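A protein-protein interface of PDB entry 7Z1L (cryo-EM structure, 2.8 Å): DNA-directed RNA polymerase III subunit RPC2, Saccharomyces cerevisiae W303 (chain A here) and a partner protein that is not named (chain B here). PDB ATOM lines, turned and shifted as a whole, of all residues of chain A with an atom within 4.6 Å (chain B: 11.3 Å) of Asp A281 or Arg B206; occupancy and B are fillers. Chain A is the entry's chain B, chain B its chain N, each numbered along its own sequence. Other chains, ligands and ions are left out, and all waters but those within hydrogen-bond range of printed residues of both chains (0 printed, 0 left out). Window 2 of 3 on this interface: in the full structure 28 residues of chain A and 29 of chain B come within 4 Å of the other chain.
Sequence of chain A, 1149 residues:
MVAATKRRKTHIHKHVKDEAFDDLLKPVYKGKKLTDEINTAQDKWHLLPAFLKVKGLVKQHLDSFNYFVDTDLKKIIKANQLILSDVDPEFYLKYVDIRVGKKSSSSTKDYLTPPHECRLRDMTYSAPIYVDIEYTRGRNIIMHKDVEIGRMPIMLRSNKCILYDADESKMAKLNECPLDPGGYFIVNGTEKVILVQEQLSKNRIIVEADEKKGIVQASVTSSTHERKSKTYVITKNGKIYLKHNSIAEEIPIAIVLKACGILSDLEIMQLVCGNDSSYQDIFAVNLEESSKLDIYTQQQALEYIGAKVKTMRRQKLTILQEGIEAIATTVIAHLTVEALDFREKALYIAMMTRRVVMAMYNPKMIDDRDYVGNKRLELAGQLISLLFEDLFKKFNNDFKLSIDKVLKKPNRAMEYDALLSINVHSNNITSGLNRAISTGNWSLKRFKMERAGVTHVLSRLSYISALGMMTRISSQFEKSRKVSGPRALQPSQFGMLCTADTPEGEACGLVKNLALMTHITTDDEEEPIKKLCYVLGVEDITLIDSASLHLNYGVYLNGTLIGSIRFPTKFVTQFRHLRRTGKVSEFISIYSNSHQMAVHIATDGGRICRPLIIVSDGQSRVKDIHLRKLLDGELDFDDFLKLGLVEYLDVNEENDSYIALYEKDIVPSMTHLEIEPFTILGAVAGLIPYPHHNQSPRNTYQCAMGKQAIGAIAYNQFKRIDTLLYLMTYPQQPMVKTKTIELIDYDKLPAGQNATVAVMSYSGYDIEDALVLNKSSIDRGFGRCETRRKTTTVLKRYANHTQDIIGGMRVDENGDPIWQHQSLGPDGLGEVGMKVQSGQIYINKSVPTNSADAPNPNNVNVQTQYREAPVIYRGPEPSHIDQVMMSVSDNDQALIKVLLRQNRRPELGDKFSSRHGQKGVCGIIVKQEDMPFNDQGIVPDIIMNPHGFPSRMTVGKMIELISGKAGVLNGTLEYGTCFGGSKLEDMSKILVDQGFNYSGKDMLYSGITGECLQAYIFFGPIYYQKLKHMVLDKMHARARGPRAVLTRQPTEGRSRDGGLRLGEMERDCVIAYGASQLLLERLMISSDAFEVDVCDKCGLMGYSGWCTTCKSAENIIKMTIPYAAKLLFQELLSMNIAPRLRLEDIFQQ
The backbone carbonyl oxygen of Val B205 lies within hydrogen-bond range of the side-chain amide nitrogen of Gln A280. The guanidinium group (NH1) of Arg B206 lies close to the side-chain amide oxygen (OE1) of Gln A280, at 3.3 Å. The backbone carbonyl oxygen (O) of Asn A275 lies within hydrogen-bond range of the backbone NH (N) of Val B207 (2.7 Å). The side-chain carboxylate (OD1) of Asp A281 is in salt-bridge range of the guanidinium group (NH2) of Arg B206. The backbone carbonyl oxygen of Val B207 lies within hydrogen-bond range of the backbone NH of Ser A277, 2.7 Å away.
The side-chain carboxylate (OD2) of Asp B211 is in salt-bridge range of the guanidinium group (NH1) of Arg B208.
Among the printed residues, pairs that only touch across the chains: Asn A275 with Val B205 (3.9 Å), Asn A275 with Arg B206 (3.6 Å), Asn A275 with Ile B219 (3.4 Å), Ser A277 with Arg B208 (3.8 Å), Ser A278 with His B209 (3.6 Å) and Tyr A279 with His B209 (3.3 Å).
Of chain B, only Arg B206 comes within 4 Å of Asp A281. Arg B206 touches three residues of chain A. Asn A275 touches just these residues of chain B: Val B205, Arg B206, Val B207 and Ile B219. Ser A277 touches just these residues of chain B: Val B207 and Arg B208. Of chain B, only His B209 comes within 4 Å of Ser A278. Gln A280 touches two residues of chain B. Printed residues of chain A within 4 Å of Ile B219: Asn A275. Of the printed residues of chain A, Val B207 touches Asn A275 and Ser A277. Glu B210 touches none of the printed residues of chain A. Lys B216 touches none of the printed residues of chain A. The nearest residue of chain A that does not touch Arg B206 is Ser A277 (4.1 Å). The nearest printed residue of chain A that does not touch His B209 is Ser A277 (4.4 Å).
Hydrophobic or aromatic side chains of chain A that line the printed part of chain B: Tyr A279. Of the 17 printed residues of chain B, 6 touch a printed residue of chain A. Hydrophobic or aromatic side chains of chain B within 4 Å of the printed part of chain A: Val B205, Val B207, His B209 and Ile B219. Among the printed residues, Asp or Glu carboxylates within 4 Å of a Lys or Arg side-chain nitrogen of the other chain: Asp A281 with Arg B206.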
ATOM      1  N   ASN A 275      -0.072  -7.282  30.383  1.00  0.00           N
ATOM      2  CA  ASN A 275      -1.139  -7.404  29.401  1.00  0.00           C
ATOM      3  C   ASN A 275      -1.744  -6.065  28.998  1.00  0.00           C
ATOM      4  O   ASN A 275      -2.584  -6.031  28.095  1.00  0.00           O
ATOM      5  CB  ASN A 275      -2.238  -8.323  29.937  1.00  0.00           C
ATOM      6  CG  ASN A 275      -1.783  -9.761  30.057  1.00  0.00           C
ATOM      7  OD1 ASN A 275      -0.717 -10.129  29.565  1.00  0.00           O
ATOM      8  ND2 ASN A 275      -2.587 -10.582  30.718  1.00  0.00           N
ATOM      9  N   SER A 277      -2.203  -2.730  27.107  1.00  0.00           N
ATOM     10  CA  SER A 277      -1.748  -2.293  25.791  1.00  0.00           C
ATOM     11  C   SER A 277      -1.091  -0.920  25.849  1.00  0.00           C
ATOM     12  O   SER A 277      -0.131  -0.657  25.114  1.00  0.00           O
ATOM     13  CB  SER A 277      -2.920  -2.282  24.811  1.00  0.00           C
ATOM     14  OG  SER A 277      -3.812  -1.222  25.104  1.00  0.00           O
ATOM     15  N   SER A 278      -1.604  -0.026  26.698  1.00  0.00           N
ATOM     16  CA  SER A 278      -1.067   1.330  26.768  1.00  0.00           C
ATOM     17  C   SER A 278       0.358   1.339  27.311  1.00  0.00           C
ATOM     18  O   SER A 278       1.209   2.095  26.825  1.00  0.00           O
ATOM     19  CB  SER A 278      -1.975   2.205  27.628  1.00  0.00           C
ATOM     20  OG  SER A 278      -3.336   2.000  27.297  1.00  0.00           O
ATOM     21  N   TYR A 279       0.635   0.502  28.314  1.00  0.00           N
ATOM     22  CA  TYR A 279       1.992   0.404  28.841  1.00  0.00           C
ATOM     23  C   TYR A 279       2.947  -0.130  27.784  1.00  0.00           C
ATOM     24  O   TYR A 279       4.089   0.331  27.679  1.00  0.00           O
ATOM     25  CB  TYR A 279       2.019  -0.484  30.087  1.00  0.00           C
ATOM     26  CG  TYR A 279       1.205   0.026  31.261  1.00  0.00           C
ATOM     27  CD1 TYR A 279       0.807   1.353  31.339  1.00  0.00           C
ATOM     28  CD2 TYR A 279       0.844  -0.826  32.294  1.00  0.00           C
ATOM     29  CE1 TYR A 279       0.065   1.814  32.408  1.00  0.00           C
ATOM     30  CE2 TYR A 279       0.104  -0.374  33.368  1.00  0.00           C
ATOM     31  CZ  TYR A 279      -0.282   0.945  33.419  1.00  0.00           C
ATOM     32  OH  TYR A 279      -1.019   1.399  34.488  1.00  0.00           O
ATOM     33  N   GLN A 280       2.493  -1.100  26.986  1.00  0.00           N
ATOM     34  CA  GLN A 280       3.313  -1.610  25.892  1.00  0.00           C
ATOM     35  C   GLN A 280       3.578  -0.532  24.852  1.00  0.00           C
ATOM     36  O   GLN A 280       4.699  -0.413  24.345  1.00  0.00           O
ATOM     37  CB  GLN A 280       2.633  -2.813  25.243  1.00  0.00           C
ATOM     38  CG  GLN A 280       2.475  -4.000  26.160  1.00  0.00           C
ATOM     39  CD  GLN A 280       1.856  -5.190  25.465  1.00  0.00           C
ATOM     40  OE1 GLN A 280       1.559  -5.139  24.273  1.00  0.00           O
ATOM     41  NE2 GLN A 280       1.655  -6.271  26.206  1.00  0.00           N
ATOM     42  N   ASP A 281       2.557   0.264  24.522  1.00  0.00           N
ATOM     43  CA  ASP A 281       2.732   1.338  23.550  1.00  0.00           C
ATOM     44  C   ASP A 281       3.724   2.381  24.051  1.00  0.00           C
ATOM     45  O   ASP A 281       4.516   2.920  23.268  1.00  0.00           O
ATOM     46  CB  ASP A 281       1.384   1.986  23.239  1.00  0.00           C
ATOM     47  CG  ASP A 281       0.444   1.053  22.501  1.00  0.00           C
ATOM     48  OD1 ASP A 281       0.873  -0.063  22.141  1.00  0.00           O
ATOM     49  OD2 ASP A 281      -0.726   1.434  22.283  1.00  0.00           O
ATOM     50  N   ILE A 282       3.689   2.682  25.349  1.00  0.00           N
ATOM     51  CA  ILE A 282       4.631   3.648  25.907  1.00  0.00           C
ATOM     52  C   ILE A 282       6.046   3.075  25.940  1.00  0.00           C
ATOM     53  O   ILE A 282       7.017   3.764  25.604  1.00  0.00           O
ATOM     54  CB  ILE A 282       4.165   4.100  27.304  1.00  0.00           C
ATOM     55  CG1 ILE A 282       2.854   4.878  27.197  1.00  0.00           C
ATOM     56  CG2 ILE A 282       5.218   4.959  27.976  1.00  0.00           C
ATOM     57  CD1 ILE A 282       2.251   5.233  28.531  1.00  0.00           C
ATOM     58  N   PHE A 283       6.188   1.805  26.321  1.00  0.00           N
ATOM     59  CA  PHE A 283       7.501   1.232  26.594  1.00  0.00           C
ATOM     60  C   PHE A 283       8.184   0.636  25.366  1.00  0.00           C
ATOM     61  O   PHE A 283       9.395   0.390  25.412  1.00  0.00           O
ATOM     62  CB  PHE A 283       7.368   0.163  27.685  1.00  0.00           C
ATOM     63  CG  PHE A 283       8.672  -0.431  28.128  1.00  0.00           C
ATOM     64  CD1 PHE A 283       9.593   0.327  28.827  1.00  0.00           C
ATOM     65  CD2 PHE A 283       8.980  -1.748  27.839  1.00  0.00           C
ATOM     66  CE1 PHE A 283      10.794  -0.217  29.230  1.00  0.00           C
ATOM     67  CE2 PHE A 283      10.180  -2.297  28.242  1.00  0.00           C
ATOM     68  CZ  PHE A 283      11.086  -1.531  28.938  1.00  0.00           C
ATOM     69  N   ALA A 284       7.460   0.431  24.260  1.00  0.00           N
ATOM     70  CA  ALA A 284       8.037  -0.246  23.102  1.00  0.00           C
ATOM     71  C   ALA A 284       9.169   0.539  22.450  1.00  0.00           C
ATOM     72  O   ALA A 284       9.937  -0.039  21.674  1.00  0.00           O
ATOM     73  CB  ALA A 284       6.948  -0.531  22.068  1.00  0.00           C
ATOM     74  N   PRO B 201       5.664 -15.515  13.739  1.00  0.00           N
ATOM     75  CA  PRO B 201       6.048 -14.492  14.726  1.00  0.00           C
ATOM     76  C   PRO B 201       5.006 -14.301  15.814  1.00  0.00           C
ATOM     77  O   PRO B 201       3.863 -13.926  15.531  1.00  0.00           O
ATOM     78  CB  PRO B 201       6.200 -13.219  13.885  1.00  0.00           C
ATOM     79  CG  PRO B 201       6.302 -13.659  12.473  1.00  0.00           C
ATOM     80  CD  PRO B 201       5.951 -15.106  12.354  1.00  0.00           C
ATOM     81  N   VAL B 202       5.393 -14.552  17.064  1.00  0.00           N
ATOM     82  CA  VAL B 202       4.433 -14.540  18.160  1.00  0.00           C
ATOM     83  C   VAL B 202       4.021 -13.105  18.473  1.00  0.00           C
ATOM     84  O   VAL B 202       4.856 -12.193  18.537  1.00  0.00           O
ATOM     85  CB  VAL B 202       5.006 -15.273  19.387  1.00  0.00           C
ATOM     86  CG1 VAL B 202       6.244 -14.580  19.946  1.00  0.00           C
ATOM     87  CG2 VAL B 202       3.942 -15.423  20.463  1.00  0.00           C
ATOM     88  N   ARG B 203       2.713 -12.890  18.601  1.00  0.00           N
ATOM     89  CA  ARG B 203       2.150 -11.600  18.971  1.00  0.00           C
ATOM     90  C   ARG B 203       1.741 -11.623  20.432  1.00  0.00           C
ATOM     91  O   ARG B 203       0.951 -12.489  20.834  1.00  0.00           O
ATOM     92  CB  ARG B 203       0.945 -11.263  18.096  1.00  0.00           C
ATOM     93  CG  ARG B 203       1.294 -11.015  16.637  1.00  0.00           C
ATOM     94  CD  ARG B 203       0.064 -10.650  15.822  1.00  0.00           C
ATOM     95  NE  ARG B 203       0.374 -10.495  14.404  1.00  0.00           N
ATOM     96  CZ  ARG B 203       0.761  -9.359  13.839  1.00  0.00           C
ATOM     97  NH1 ARG B 203       0.885  -8.245  14.542  1.00  0.00           N
ATOM     98  NH2 ARG B 203       1.030  -9.340  12.538  1.00  0.00           N
ATOM     99  N   PRO B 204       2.256 -10.707  21.248  1.00  0.00           N
ATOM    100  CA  PRO B 204       1.974 -10.753  22.686  1.00  0.00           C
ATOM    101  C   PRO B 204       0.534 -10.388  23.001  1.00  0.00           C
ATOM    102  O   PRO B 204      -0.169  -9.750  22.214  1.00  0.00           O
ATOM    103  CB  PRO B 204       2.943  -9.720  23.262  1.00  0.00           C
ATOM    104  CG  PRO B 204       3.127  -8.743  22.151  1.00  0.00           C
ATOM    105  CD  PRO B 204       3.094  -9.553  20.885  1.00  0.00           C
ATOM    106  N   VAL B 205       0.098 -10.816  24.187  1.00  0.00           N
ATOM    107  CA  VAL B 205      -1.264 -10.553  24.632  1.00  0.00           C
ATOM    108  C   VAL B 205      -1.425  -9.068  24.921  1.00  0.00           C
ATOM    109  O   VAL B 205      -0.671  -8.486  25.712  1.00  0.00           O
ATOM    110  CB  VAL B 205      -1.595 -11.400  25.870  1.00  0.00           C
ATOM    111  CG1 VAL B 205      -2.912 -10.956  26.482  1.00  0.00           C
ATOM    112  CG2 VAL B 205      -1.641 -12.874  25.505  1.00  0.00           C
ATOM    113  N   ARG B 206      -2.410  -8.445  24.277  1.00  0.00           N
ATOM    114  CA  ARG B 206      -2.688  -7.027  24.453  1.00  0.00           C
ATOM    115  C   ARG B 206      -4.120  -6.855  24.931  1.00  0.00           C
ATOM    116  O   ARG B 206      -5.055  -7.354  24.296  1.00  0.00           O
ATOM    117  CB  ARG B 206      -2.469  -6.252  23.151  1.00  0.00           C
ATOM    118  CG  ARG B 206      -1.046  -6.298  22.632  1.00  0.00           C
ATOM    119  CD  ARG B 206      -0.960  -5.732  21.227  1.00  0.00           C
ATOM    120  NE  ARG B 206      -1.291  -4.314  21.195  1.00  0.00           N
ATOM    121  CZ  ARG B 206      -0.401  -3.336  21.286  1.00  0.00           C
ATOM    122  NH1 ARG B 206       0.892  -3.587  21.408  1.00  0.00           N
ATOM    123  NH2 ARG B 206      -0.819  -2.073  21.254  1.00  0.00           N
ATOM    124  N   VAL B 207      -4.287  -6.151  26.047  1.00  0.00           N
ATOM    125  CA  VAL B 207      -5.599  -5.852  26.609  1.00  0.00           C
ATOM    126  C   VAL B 207      -5.691  -4.347  26.812  1.00  0.00           C
ATOM    127  O   VAL B 207      -4.713  -3.705  27.207  1.00  0.00           O
ATOM    128  CB  VAL B 207      -5.841  -6.601  27.939  1.00  0.00           C
ATOM    129  CG1 VAL B 207      -7.258  -6.370  28.435  1.00  0.00           C
ATOM    130  CG2 VAL B 207      -5.573  -8.090  27.784  1.00  0.00           C
ATOM    131  N   ARG B 208      -6.863  -3.784  26.526  1.00  0.00           N
ATOM    132  CA  ARG B 208      -7.089  -2.363  26.747  1.00  0.00           C
ATOM    133  C   ARG B 208      -6.984  -2.034  28.233  1.00  0.00           C
ATOM    134  O   ARG B 208      -7.242  -2.876  29.097  1.00  0.00           O
ATOM    135  CB  ARG B 208      -8.458  -1.955  26.202  1.00  0.00           C
ATOM    136  CG  ARG B 208      -8.573  -2.088  24.692  1.00  0.00           C
ATOM    137  CD  ARG B 208      -9.951  -1.696  24.186  1.00  0.00           C
ATOM    138  NE  ARG B 208     -10.232  -0.279  24.374  1.00  0.00           N
ATOM    139  CZ  ARG B 208     -11.106   0.202  25.247  1.00  0.00           C
ATOM    140  NH1 ARG B 208     -11.810  -0.598  26.032  1.00  0.00           N
ATOM    141  NH2 ARG B 208     -11.280   1.518  25.334  1.00  0.00           N
ATOM    142  N   HIS B 209      -6.582  -0.793  28.521  1.00  0.00           N
ATOM    143  CA  HIS B 209      -6.250  -0.408  29.890  1.00  0.00           C
ATOM    144  C   HIS B 209      -7.471  -0.435  30.800  1.00  0.00           C
ATOM    145  O   HIS B 209      -7.363  -0.777  31.983  1.00  0.00           O
ATOM    146  CB  HIS B 209      -5.609   0.979  29.903  1.00  0.00           C
ATOM    147  CG  HIS B 209      -5.196   1.438  31.266  1.00  0.00           C
ATOM    148  ND1 HIS B 209      -4.113   0.909  31.933  1.00  0.00           N
ATOM    149  CD2 HIS B 209      -5.726   2.371  32.090  1.00  0.00           C
ATOM    150  CE1 HIS B 209      -3.990   1.500  33.107  1.00  0.00           C
ATOM    151  NE2 HIS B 209      -4.956   2.392  33.228  1.00  0.00           N
ATOM    152  N   GLU B 210      -8.640  -0.071  30.274  1.00  0.00           N
ATOM    153  CA  GLU B 210      -9.841  -0.063  31.100  1.00  0.00           C
ATOM    154  C   GLU B 210     -10.348  -1.469  31.402  1.00  0.00           C
ATOM    155  O   GLU B 210     -11.138  -1.641  32.336  1.00  0.00           O
ATOM    156  CB  GLU B 210     -10.938   0.759  30.418  1.00  0.00           C
ATOM    157  CG  GLU B 210     -11.984   1.322  31.371  1.00  0.00           C
ATOM    158  CD  GLU B 210     -11.405   2.325  32.351  1.00  0.00           C
ATOM    159  OE1 GLU B 210     -10.473   3.066  31.970  1.00  0.00           O
ATOM    160  OE2 GLU B 210     -11.881   2.373  33.504  1.00  0.00           O
ATOM    161  N   ASP B 211      -9.908  -2.474  30.647  1.00  0.00           N
ATOM    162  CA  ASP B 211     -10.394  -3.839  30.802  1.00  0.00           C
ATOM    163  C   ASP B 211      -9.356  -4.782  31.397  1.00  0.00           C
ATOM    164  O   ASP B 211      -9.599  -5.993  31.448  1.00  0.00           O
ATOM    165  CB  ASP B 211     -10.873  -4.382  29.454  1.00  0.00           C
ATOM    166  CG  ASP B 211     -11.843  -3.447  28.759  1.00  0.00           C
ATOM    167  OD1 ASP B 211     -12.529  -2.672  29.458  1.00  0.00           O
ATOM    168  OD2 ASP B 211     -11.921  -3.488  27.513  1.00  0.00           O
ATOM    169  N   VAL B 212      -8.206  -4.268  31.843  1.00  0.00           N
ATOM    170  CA  VAL B 212      -7.148  -5.151  32.331  1.00  0.00           C
ATOM    171  C   VAL B 212      -7.527  -5.778  33.670  1.00  0.00           C
ATOM    172  O   VAL B 212      -7.140  -6.917  33.962  1.00  0.00           O
ATOM    173  CB  VAL B 212      -5.802  -4.392  32.398  1.00  0.00           C
ATOM    174  CG1 VAL B 212      -5.839  -3.267  33.424  1.00  0.00           C
ATOM    175  CG2 VAL B 212      -4.649  -5.351  32.676  1.00  0.00           C
ATOM    176  N   GLU B 213      -8.303  -5.069  34.494  1.00  0.00           N
ATOM    177  CA  GLU B 213      -8.704  -5.607  35.787  1.00  0.00           C
ATOM    178  C   GLU B 213      -9.883  -6.566  35.688  1.00  0.00           C
ATOM    179  O   GLU B 213     -10.151  -7.296  36.648  1.00  0.00           O
ATOM    180  CB  GLU B 213      -9.048  -4.469  36.751  1.00  0.00           C
ATOM    181  CG  GLU B 213      -7.849  -3.646  37.199  1.00  0.00           C
ATOM    182  CD  GLU B 213      -7.637  -2.410  36.346  1.00  0.00           C
ATOM    183  OE1 GLU B 213      -8.454  -2.169  35.432  1.00  0.00           O
ATOM    184  OE2 GLU B 213      -6.654  -1.681  36.589  1.00  0.00           O
ATOM    185  N   VAL B 215     -10.423  -8.702  32.695  1.00  0.00           N
ATOM    186  CA  VAL B 215     -10.046  -9.876  31.910  1.00  0.00           C
ATOM    187  C   VAL B 215      -9.205 -10.862  32.710  1.00  0.00           C
ATOM    188  O   VAL B 215      -8.988 -11.991  32.253  1.00  0.00           O
ATOM    189  CB  VAL B 215      -9.293  -9.400  30.650  1.00  0.00           C
ATOM    190  CG1 VAL B 215      -7.938  -8.814  31.031  1.00  0.00           C
ATOM    191  CG2 VAL B 215      -9.191 -10.486  29.571  1.00  0.00           C
ATOM    192  N   LYS B 216      -8.751 -10.472  33.906  1.00  0.00           N
ATOM    193  CA  LYS B 216      -7.833 -11.309  34.678  1.00  0.00           C
ATOM    194  C   LYS B 216      -8.470 -12.639  35.059  1.00  0.00           C
ATOM    195  O   LYS B 216      -7.791 -13.672  35.091  1.00  0.00           O
ATOM    196  CB  LYS B 216      -7.368 -10.557  35.925  1.00  0.00           C
ATOM    197  CG  LYS B 216      -6.103  -9.743  35.712  1.00  0.00           C
ATOM    198  CD  LYS B 216      -5.941  -8.672  36.777  1.00  0.00           C
ATOM    199  CE  LYS B 216      -4.626  -7.930  36.611  1.00  0.00           C
ATOM    200  NZ  LYS B 216      -4.255  -7.771  35.178  1.00  0.00           N
ATOM    201  N   GLU B 218     -10.823 -14.217  33.187  1.00  0.00           N
ATOM    202  CA  GLU B 218     -10.866 -14.996  31.953  1.00  0.00           C
ATOM    203  C   GLU B 218      -9.484 -15.504  31.564  1.00  0.00           C
ATOM    204  O   GLU B 218      -9.336 -16.662  31.164  1.00  0.00           O
ATOM    205  CB  GLU B 218     -11.468 -14.157  30.827  1.00  0.00           C
ATOM    206  CG  GLU B 218     -11.417 -14.822  29.460  1.00  0.00           C
ATOM    207  CD  GLU B 218     -12.181 -14.047  28.405  1.00  0.00           C
ATOM    208  OE1 GLU B 218     -12.673 -12.942  28.718  1.00  0.00           O
ATOM    209  OE2 GLU B 218     -12.293 -14.543  27.266  1.00  0.00           O
ATOM    210  N   ILE B 219      -8.460 -14.656  31.686  1.00  0.00           N
ATOM    211  CA  ILE B 219      -7.102 -15.066  31.337  1.00  0.00           C
ATOM    212  C   ILE B 219      -6.603 -16.145  32.293  1.00  0.00           C
ATOM    213  O   ILE B 219      -5.990 -17.136  31.869  1.00  0.00           O
ATOM    214  CB  ILE B 219      -6.174 -13.837  31.314  1.00  0.00           C
ATOM    215  CG1 ILE B 219      -6.409 -13.027  30.039  1.00  0.00           C
ATOM    216  CG2 ILE B 219      -4.712 -14.247  31.408  1.00  0.00           C
ATOM    217  CD1 ILE B 219      -5.672 -11.712  30.009  1.00  0.00           C
